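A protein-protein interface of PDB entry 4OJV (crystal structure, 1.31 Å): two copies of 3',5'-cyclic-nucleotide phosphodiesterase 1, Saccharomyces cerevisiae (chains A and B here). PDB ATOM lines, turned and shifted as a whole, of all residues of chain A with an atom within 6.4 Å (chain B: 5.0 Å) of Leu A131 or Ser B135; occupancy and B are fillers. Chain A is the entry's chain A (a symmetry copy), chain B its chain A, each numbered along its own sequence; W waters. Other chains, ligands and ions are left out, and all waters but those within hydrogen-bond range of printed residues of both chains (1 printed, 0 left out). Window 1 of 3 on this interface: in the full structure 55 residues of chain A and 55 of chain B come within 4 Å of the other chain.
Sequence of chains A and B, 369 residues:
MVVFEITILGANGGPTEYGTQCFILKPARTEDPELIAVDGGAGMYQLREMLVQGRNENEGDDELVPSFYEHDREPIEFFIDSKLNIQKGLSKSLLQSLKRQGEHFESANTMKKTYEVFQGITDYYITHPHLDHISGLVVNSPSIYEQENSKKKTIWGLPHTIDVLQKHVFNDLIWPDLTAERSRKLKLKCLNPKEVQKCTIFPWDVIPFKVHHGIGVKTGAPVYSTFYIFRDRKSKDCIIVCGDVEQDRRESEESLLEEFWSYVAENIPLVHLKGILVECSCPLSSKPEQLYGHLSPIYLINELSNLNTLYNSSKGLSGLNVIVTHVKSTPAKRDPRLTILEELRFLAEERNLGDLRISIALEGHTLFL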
ATOM      1  N   GLU A  17      29.314  10.158  -0.347  1.00  0.00           N
ATOM      2  CA  GLU A  17      29.879  10.075   0.989  1.00  0.00           C
ATOM      3  C   GLU A  17      31.267  10.709   1.167  1.00  0.00           C
ATOM      4  O   GLU A  17      31.742  10.805   2.298  1.00  0.00           O
ATOM      5  CB  GLU A  17      29.872   8.620   1.469  1.00  0.00           C
ATOM      6  CG  GLU A  17      30.944   7.730   0.852  1.00  0.00           C
ATOM      7  CD  GLU A  17      30.628   7.208  -0.548  1.00  0.00           C
ATOM      8  OE1 GLU A  17      31.479   6.451  -1.053  1.00  0.00           O
ATOM      9  OE2 GLU A  17      29.563   7.525  -1.134  1.00  0.00           O
ATOM     10  N   THR A  20      32.558  15.494   2.355  1.00  0.00           N
ATOM     11  CA  THR A  20      31.542  16.134   3.193  1.00  0.00           C
ATOM     12  C   THR A  20      32.188  17.215   4.081  1.00  0.00           C
ATOM     13  O   THR A  20      33.405  17.403   4.066  1.00  0.00           O
ATOM     14  CB  THR A  20      30.692  15.112   3.970  1.00  0.00           C
ATOM     15  OG1 THR A  20      31.543  14.300   4.761  1.00  0.00           O
ATOM     16  CG2 THR A  20      29.901  14.217   3.020  1.00  0.00           C
ATOM     17  N   GLY A  40      34.355  18.191  10.341  1.00  0.00           N
ATOM     18  CA  GLY A  40      35.263  17.063  10.306  1.00  0.00           C
ATOM     19  C   GLY A  40      34.822  15.995   9.339  1.00  0.00           C
ATOM     20  O   GLY A  40      35.060  14.809   9.573  1.00  0.00           O
ATOM     21  N   GLY A  41      34.218  16.409   8.228  1.00  0.00           N
ATOM     22  CA  GLY A  41      33.958  15.500   7.107  1.00  0.00           C
ATOM     23  C   GLY A  41      35.285  15.237   6.376  1.00  0.00           C
ATOM     24  O   GLY A  41      36.159  14.536   6.904  1.00  0.00           O
ATOM     25  N   HIS A 128      27.726  20.051  14.537  1.00  0.00           N
ATOM     26  CA  HIS A 128      26.769  19.051  15.005  1.00  0.00           C
ATOM     27  C   HIS A 128      27.322  17.691  14.690  1.00  0.00           C
ATOM     28  O   HIS A 128      28.207  17.574  13.841  1.00  0.00           O
ATOM     29  CB  HIS A 128      25.357  19.279  14.445  1.00  0.00           C
ATOM     30  CG  HIS A 128      25.206  19.038  12.950  1.00  0.00           C
ATOM     31  ND1 HIS A 128      25.865  19.754  11.999  1.00  0.00           N
ATOM     32  CD2 HIS A 128      24.383  18.143  12.270  1.00  0.00           C
ATOM     33  CE1 HIS A 128      25.462  19.334  10.770  1.00  0.00           C
ATOM     34  NE2 HIS A 128      24.550  18.353  10.935  1.00  0.00           N
ATOM     35  N   PRO A 129      26.840  16.640  15.375  1.00  0.00           N
ATOM     36  CA  PRO A 129      27.495  15.339  15.292  1.00  0.00           C
ATOM     37  C   PRO A 129      26.927  14.396  14.230  1.00  0.00           C
ATOM     38  O   PRO A 129      27.238  13.211  14.239  1.00  0.00           O
ATOM     39  CB  PRO A 129      27.290  14.776  16.695  1.00  0.00           C
ATOM     40  CG  PRO A 129      25.932  15.287  17.062  1.00  0.00           C
ATOM     41  CD  PRO A 129      25.874  16.684  16.492  1.00  0.00           C
ATOM     42  N   HIS A 130      26.150  14.908  13.275  1.00  0.00           N
ATOM     43  CA  HIS A 130      25.767  14.061  12.132  1.00  0.00           C
ATOM     44  C   HIS A 130      27.005  13.515  11.470  1.00  0.00           C
ATOM     45  O   HIS A 130      28.030  14.206  11.346  1.00  0.00           O
ATOM     46  CB  HIS A 130      24.946  14.806  11.085  1.00  0.00           C
ATOM     47  CG  HIS A 130      23.479  14.924  11.406  1.00  0.00           C
ATOM     48  ND1 HIS A 130      22.681  15.872  10.827  1.00  0.00           N
ATOM     49  CD2 HIS A 130      22.669  14.162  12.231  1.00  0.00           C
ATOM     50  CE1 HIS A 130      21.423  15.704  11.287  1.00  0.00           C
ATOM     51  NE2 HIS A 130      21.424  14.673  12.158  1.00  0.00           N
ATOM     52  N   LEU A 131      26.914  12.258  11.038  1.00  0.00           N
ATOM     53  CA  LEU A 131      28.097  11.531  10.597  1.00  0.00           C
ATOM     54  C   LEU A 131      28.887  12.245   9.481  1.00  0.00           C
ATOM     55  O   LEU A 131      30.122  12.169   9.471  1.00  0.00           O
ATOM     56  CB  LEU A 131      27.719  10.089  10.221  1.00  0.00           C
ATOM     57  CG  LEU A 131      28.880   9.100  10.015  1.00  0.00           C
ATOM     58  CD1 LEU A 131      28.504   7.715  10.541  1.00  0.00           C
ATOM     59  CD2 LEU A 131      29.291   9.041   8.553  1.00  0.00           C
ATOM     60  N   ASP A 132      28.195  12.920   8.554  1.00  0.00           N
ATOM     61  CA  ASP A 132      28.871  13.635   7.463  1.00  0.00           C
ATOM     62  C   ASP A 132      29.750  14.787   7.945  1.00  0.00           C
ATOM     63  O   ASP A 132      30.592  15.270   7.189  1.00  0.00           O
ATOM     64  CB  ASP A 132      27.901  14.115   6.346  1.00  0.00           C
ATOM     65  CG  ASP A 132      26.777  15.047   6.865  1.00  0.00           C
ATOM     66  OD1 ASP A 132      26.170  14.657   7.892  1.00  0.00           O
ATOM     67  OD2 ASP A 132      26.459  16.169   6.297  1.00  0.00           O
ATOM     68  N   HIS A 133      29.589  15.212   9.200  1.00  0.00           N
ATOM     69  CA  HIS A 133      30.386  16.305   9.755  1.00  0.00           C
ATOM     70  C   HIS A 133      31.486  15.822  10.651  1.00  0.00           C
ATOM     71  O   HIS A 133      32.251  16.637  11.164  1.00  0.00           O
ATOM     72  CB  HIS A 133      29.493  17.334  10.465  1.00  0.00           C
ATOM     73  CG  HIS A 133      28.526  17.991   9.524  1.00  0.00           C
ATOM     74  ND1 HIS A 133      28.642  19.273   9.082  1.00  0.00           N
ATOM     75  CD2 HIS A 133      27.440  17.454   8.870  1.00  0.00           C
ATOM     76  CE1 HIS A 133      27.660  19.519   8.201  1.00  0.00           C
ATOM     77  NE2 HIS A 133      26.939  18.405   8.059  1.00  0.00           N
ATOM     78  N   ILE A 134      31.614  14.503  10.806  1.00  0.00           N
ATOM     79  CA  ILE A 134      32.626  13.948  11.712  1.00  0.00           C
ATOM     80  C   ILE A 134      33.392  12.743  11.166  1.00  0.00           C
ATOM     81  O   ILE A 134      34.312  12.275  11.814  1.00  0.00           O
ATOM     82  CB  ILE A 134      32.048  13.572  13.100  1.00  0.00           C
ATOM     83  CG1 ILE A 134      30.995  12.463  12.942  1.00  0.00           C
ATOM     84  CG2 ILE A 134      31.514  14.815  13.796  1.00  0.00           C
ATOM     85  CD1 ILE A 134      30.583  11.793  14.235  1.00  0.00           C
ATOM     86  N   SER A 135      33.026  12.241   9.990  1.00  0.00           N
ATOM     87  CA  SER A 135      33.597  10.985   9.496  1.00  0.00           C
ATOM     88  C   SER A 135      35.119  11.041   9.299  1.00  0.00           C
ATOM     89  O   SER A 135      35.820  10.080   9.641  1.00  0.00           O
ATOM     90  CB  SER A 135      32.896  10.552   8.214  1.00  0.00           C
ATOM     91  OG  SER A 135      32.973  11.556   7.237  1.00  0.00           O
ATOM     92  N   GLY A 136      35.630  12.150   8.759  1.00  0.00           N
ATOM     93  CA  GLY A 136      37.070  12.311   8.586  1.00  0.00           C
ATOM     94  C   GLY A 136      37.792  12.506   9.904  1.00  0.00           C
ATOM     95  O   GLY A 136      38.825  11.887  10.149  1.00  0.00           O
ATOM     96  N   VAL A 139      37.855   8.838  11.378  1.00  0.00           N
ATOM     97  CA  VAL A 139      38.722   7.851  10.732  1.00  0.00           C
ATOM     98  C   VAL A 139      40.189   8.310  10.737  1.00  0.00           C
ATOM     99  O   VAL A 139      41.097   7.486  10.870  1.00  0.00           O
ATOM    100  CB  VAL A 139      38.201   7.472   9.339  1.00  0.00           C
ATOM    101  CG1 VAL A 139      39.145   6.489   8.661  1.00  0.00           C
ATOM    102  CG2 VAL A 139      36.795   6.876   9.449  1.00  0.00           C
ATOM    103  N   ILE A 174      31.410   2.258  18.080  1.00  0.00           N
ATOM    104  CA  ILE A 174      31.501   2.965  16.800  1.00  0.00           C
ATOM    105  C   ILE A 174      32.960   3.316  16.479  1.00  0.00           C
ATOM    106  O   ILE A 174      33.377   3.328  15.317  1.00  0.00           O
ATOM    107  CB  ILE A 174      30.592   4.215  16.826  1.00  0.00           C
ATOM    108  CG1 ILE A 174      29.112   3.798  16.891  1.00  0.00           C
ATOM    109  CG2 ILE A 174      30.883   5.144  15.644  1.00  0.00           C
ATOM    110  CD1 ILE A 174      28.639   2.971  15.718  1.00  0.00           C
ATOM    111  N   THR B  20      37.122   3.409   2.298  1.00  0.00           N
ATOM    112  CA  THR B  20      37.175   2.396   3.354  1.00  0.00           C
ATOM    113  C   THR B  20      36.257   1.210   3.002  1.00  0.00           C
ATOM    114  O   THR B  20      35.565   1.227   1.983  1.00  0.00           O
ATOM    115  CB  THR B  20      36.921   2.992   4.752  1.00  0.00           C
ATOM    116  OG1 THR B  20      35.663   3.645   4.760  1.00  0.00           O
ATOM    117  CG2 THR B  20      38.003   3.999   5.128  1.00  0.00           C
ATOM    118  N   GLY B  40      30.198  -1.271   4.401  1.00  0.00           N
ATOM    119  CA  GLY B  40      29.505  -0.060   4.013  1.00  0.00           C
ATOM    120  C   GLY B  40      30.363   1.169   4.157  1.00  0.00           C
ATOM    121  O   GLY B  40      29.854   2.251   4.458  1.00  0.00           O
ATOM    122  N   GLY B  41      31.662   1.024   3.903  1.00  0.00           N
ATOM    123  CA  GLY B  41      32.557   2.179   3.775  1.00  0.00           C
ATOM    124  C   GLY B  41      32.290   2.851   2.418  1.00  0.00           C
ATOM    125  O   GLY B  41      31.243   3.486   2.232  1.00  0.00           O
ATOM    126  N   LEU B 131      33.215   2.949  12.409  1.00  0.00           N
ATOM    127  CA  LEU B 131      32.737   3.950  11.465  1.00  0.00           C
ATOM    128  C   LEU B 131      33.246   3.739  10.024  1.00  0.00           C
ATOM    129  O   LEU B 131      32.499   4.004   9.073  1.00  0.00           O
ATOM    130  CB  LEU B 131      33.036   5.360  11.993  1.00  0.00           C
ATOM    131  CG  LEU B 131      32.347   6.532  11.272  1.00  0.00           C
ATOM    132  CD1 LEU B 131      31.948   7.617  12.272  1.00  0.00           C
ATOM    133  CD2 LEU B 131      33.236   7.095  10.176  1.00  0.00           C
ATOM    134  N   ASP B 132      34.492   3.278   9.858  1.00  0.00           N
ATOM    135  CA  ASP B 132      35.050   3.040   8.520  1.00  0.00           C
ATOM    136  C   ASP B 132      34.321   1.946   7.743  1.00  0.00           C
ATOM    137  O   ASP B 132      34.482   1.851   6.527  1.00  0.00           O
ATOM    138  CB  ASP B 132      36.585   2.779   8.530  1.00  0.00           C
ATOM    139  CG  ASP B 132      36.998   1.571   9.409  1.00  0.00           C
ATOM    140  OD1 ASP B 132      36.498   1.532  10.559  1.00  0.00           O
ATOM    141  OD2 ASP B 132      37.806   0.639   9.010  1.00  0.00           O
ATOM    142  N   HIS B 133      33.501   1.141   8.421  1.00  0.00           N
ATOM    143  CA  HIS B 133      32.755   0.067   7.765  1.00  0.00           C
ATOM    144  C   HIS B 133      31.316   0.420   7.536  1.00  0.00           C
ATOM    145  O   HIS B 133      30.580  -0.384   6.967  1.00  0.00           O
ATOM    146  CB  HIS B 133      32.895  -1.252   8.538  1.00  0.00           C
ATOM    147  CG  HIS B 133      34.315  -1.734   8.587  1.00  0.00           C
ATOM    148  ND1 HIS B 133      34.789  -2.788   7.867  1.00  0.00           N
ATOM    149  CD2 HIS B 133      35.399  -1.198   9.246  1.00  0.00           C
ATOM    150  CE1 HIS B 133      36.108  -2.904   8.085  1.00  0.00           C
ATOM    151  NE2 HIS B 133      36.482  -1.924   8.911  1.00  0.00           N
ATOM    152  N   ILE B 134      30.915   1.633   7.920  1.00  0.00           N
ATOM    153  CA  ILE B 134      29.510   2.037   7.786  1.00  0.00           C
ATOM    154  C   ILE B 134      29.291   3.453   7.255  1.00  0.00           C
ATOM    155  O   ILE B 134      28.158   3.838   7.027  1.00  0.00           O
ATOM    156  CB  ILE B 134      28.712   1.880   9.106  1.00  0.00           C
ATOM    157  CG1 ILE B 134      29.298   2.808  10.181  1.00  0.00           C
ATOM    158  CG2 ILE B 134      28.680   0.418   9.524  1.00  0.00           C
ATOM    159  CD1 ILE B 134      28.430   2.983  11.408  1.00  0.00           C
ATOM    160  N   SER B 135      30.356   4.225   7.057  1.00  0.00           N
ATOM    161  CA  SER B 135      30.205   5.644   6.722  1.00  0.00           C
ATOM    162  C   SER B 135      29.453   5.886   5.406  1.00  0.00           C
ATOM    163  O   SER B 135      28.615   6.794   5.333  1.00  0.00           O
ATOM    164  CB  SER B 135      31.565   6.331   6.708  1.00  0.00           C
ATOM    165  OG  SER B 135      32.439   5.695   5.814  1.00  0.00           O
ATOM    166  N   GLY B 136      29.740   5.085   4.376  1.00  0.00           N
ATOM    167  CA  GLY B 136      29.034   5.209   3.106  1.00  0.00           C
ATOM    168  C   GLY B 136      27.596   4.737   3.195  1.00  0.00           C
ATOM    169  O   GLY B 136      26.687   5.403   2.705  1.00  0.00           O
ATOM    170  N   LEU B 137      27.380   3.590   3.831  1.00  0.00           N
ATOM    171  CA  LEU B 137      26.032   3.120   4.093  1.00  0.00           C
ATOM    172  C   LEU B 137      25.189   4.244   4.703  1.00  0.00           C
ATOM    173  O   LEU B 137      24.063   4.504   4.272  1.00  0.00           O
ATOM    174  CB  LEU B 137      26.086   1.920   5.052  1.00  0.00           C
ATOM    175  CG  LEU B 137      24.808   1.556   5.812  1.00  0.00           C
ATOM    176  CD1 LEU B 137      23.693   1.076   4.894  1.00  0.00           C
ATOM    177  CD2 LEU B 137      25.110   0.522   6.890  1.00  0.00           C
ATOM    178  N   VAL B 138      25.738   4.897   5.724  1.00  0.00           N
ATOM    179  CA  VAL B 138      24.988   5.921   6.427  1.00  0.00           C
ATOM    180  C   VAL B 138      24.764   7.163   5.564  1.00  0.00           C
ATOM    181  O   VAL B 138      23.626   7.591   5.363  1.00  0.00           O
ATOM    182  CB  VAL B 138      25.680   6.275   7.757  1.00  0.00           C
ATOM    183  CG1 VAL B 138      25.015   7.481   8.405  1.00  0.00           C
ATOM    184  CG2 VAL B 138      25.659   5.079   8.705  1.00  0.00           C
ATOM    185  N   VAL B 139      25.837   7.748   5.056  1.00  0.00           N
ATOM    186  CA  VAL B 139      25.671   9.006   4.327  1.00  0.00           C
ATOM    187  C   VAL B 139      24.854   8.800   3.041  1.00  0.00           C
ATOM    188  O   VAL B 139      24.077   9.674   2.651  1.00  0.00           O
ATOM    189  CB  VAL B 139      27.017   9.704   4.095  1.00  0.00           C
ATOM    190  CG1 VAL B 139      26.829  10.981   3.285  1.00  0.00           C
ATOM    191  CG2 VAL B 139      27.684  10.015   5.437  1.00  0.00           C
ATOM    192  N   ASN B 140      24.991   7.628   2.405  1.00  0.00           N
ATOM    193  CA  ASN B 140      24.248   7.336   1.175  1.00  0.00           C
ATOM    194  C   ASN B 140      22.758   7.079   1.436  1.00  0.00           C
ATOM    195  O   ASN B 140      21.953   7.176   0.512  1.00  0.00           O
ATOM    196  CB  ASN B 140      24.764   6.078   0.447  1.00  0.00           C
ATOM    197  CG  ASN B 140      26.196   6.159  -0.073  1.00  0.00           C
ATOM    198  OD1 ASN B 140      26.729   5.118  -0.457  1.00  0.00           O
ATOM    199  ND2 ASN B 140      26.802   7.332  -0.136  1.00  0.00           N
ATOM    200  N   ILE B 174      23.450  10.911  15.736  1.00  0.00           N
ATOM    201  CA  ILE B 174      24.507  10.649  14.756  1.00  0.00           C
ATOM    202  C   ILE B 174      23.934  10.640  13.333  1.00  0.00           C
ATOM    203  O   ILE B 174      24.596  11.045  12.372  1.00  0.00           O
ATOM    204  CB  ILE B 174      25.226   9.324  15.104  1.00  0.00           C
ATOM    205  CG1 ILE B 174      26.001   9.469  16.426  1.00  0.00           C
ATOM    206  CG2 ILE B 174      26.121   8.854  13.953  1.00  0.00           C
ATOM    207  CD1 ILE B 174      27.078  10.529  16.411  1.00  0.00           C
ATOM    208  N   TRP B 175      22.693  10.187  13.203  1.00  0.00           N
ATOM    209  CA  TRP B 175      22.000  10.176  11.916  1.00  0.00           C
ATOM    210  C   TRP B 175      20.520  10.140  12.162  1.00  0.00           C
ATOM    211  O   TRP B 175      20.090   9.529  13.145  1.00  0.00           O
ATOM    212  CB  TRP B 175      22.409   8.949  11.100  1.00  0.00           C
ATOM    213  CG  TRP B 175      22.190   9.135   9.627  1.00  0.00           C
ATOM    214  CD1 TRP B 175      21.301   8.463   8.801  1.00  0.00           C
ATOM    215  CD2 TRP B 175      22.903  10.075   8.772  1.00  0.00           C
ATOM    216  NE1 TRP B 175      21.405   8.926   7.505  1.00  0.00           N
ATOM    217  CE2 TRP B 175      22.363   9.899   7.428  1.00  0.00           C
ATOM    218  CE3 TRP B 175      23.899  11.018   8.989  1.00  0.00           C
ATOM    219  CZ2 TRP B 175      22.834  10.636   6.350  1.00  0.00           C
ATOM    220  CZ3 TRP B 175      24.353  11.765   7.903  1.00  0.00           C
ATOM    221  CH2 TRP B 175      23.838  11.571   6.615  1.00  0.00           C
HETATM  222  O   HOH W   1      32.199   8.899   4.434  1.00  0.00           O
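Ser B135 touches one residue of chain A. Of the printed residues of chain B, Asp A132 touches Trp B175 (3.4 Å). Of the printed residues of chain A, Trp B175 touches Leu A131 (3.9 Å) and Asp A132 (3.4 Å). The nearest residue of chain A that does not touch Ser B135 is Glu A17 (4.5 Å).
Water W1 lies within hydrogen-bond range of the backbone carbonyl oxygen (O) of Glu A17 and the side-chain hydroxyl (OG) of Ser B135.
Of the 15 printed residues of chain A, 8 touch a printed residue of chain B. Printed residues of chain A that touch a printed residue of chain B: Glu A17, Pro A129, His A130, Leu A131, Asp A132, Ser A135, Val A139 and Ile A174. Printed residues of chain B that touch a printed residue of chain A: Leu B131, Ser B135, Gly B136, Val B139, Asn B140, Ile B174 and Trp B175. Among the printed residues, no Asp or Glu carboxylate lies within 4 Å of a Lys or Arg side-chain nitrogen of the other chain.
Leu B131 touches its own counterpart, Leu A131. Leu A131 touches Ser B135, and with the chains exchanged Ser A135 touches Leu B131. Leu A131 touches Val B139, and with the chains exchanged Val A139 touches Leu B131. Leu A131 touches Ile B174, and with the chains exchanged Ile A174 touches Leu B131. Positions printed for both chains: 20, 40, 41, 131, 132, 133, 134, 135, 136, 139 and 174.
Among the printed residues, pairs that only touch across the chains: His A130 with Ile B174, Asp A132 with Trp B175, Pro A129 with Ile B174, Leu A131 with Val B139, Val A139 with Leu B131, Leu A131 with Trp B175, Leu A131 with Leu B131, Glu A17 with Gly B136, Glu A17 with Val B139, Ser A135 with Leu B131 and Leu A131 with Ser B135.
O of Ile B174 lies within hydrogen-bond range of N of Leu A131, at 2.9 Å. The backbone carbonyl oxygen of Ile A174 is in hydrogen-bond range of the backbone NH of Leu B131. The side-chain amide nitrogen (ND2) of Asn B140 sits at hydrogen-bond distance from the side-chain carboxylate (OE2) of Glu A17.
The backbone carbonyl oxygen (O) of Gly A40 sits at hydrogen-bond distance from the backbone NH (N) of Ser A135, 3.3 Å away. The backbone carbonyl oxygen of Gly B40 sits at hydrogen-bond distance from the backbone NH of Gly B136 (2.8 Å). The backbone carbonyl oxygen (O) of Gly B41 sits close to the backbone NH (N) of Gly B136. O of Gly B40 is in hydrogen-bond range of N of Ser B135 (3.3 Å). The indole nitrogen (NE1) of Trp B175 lies close to the backbone carbonyl oxygen (O) of Val B138, at 3.4 Å. OG1 of Thr A20 is in hydrogen-bond range of O of Asp A132, 2.8 Å away.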
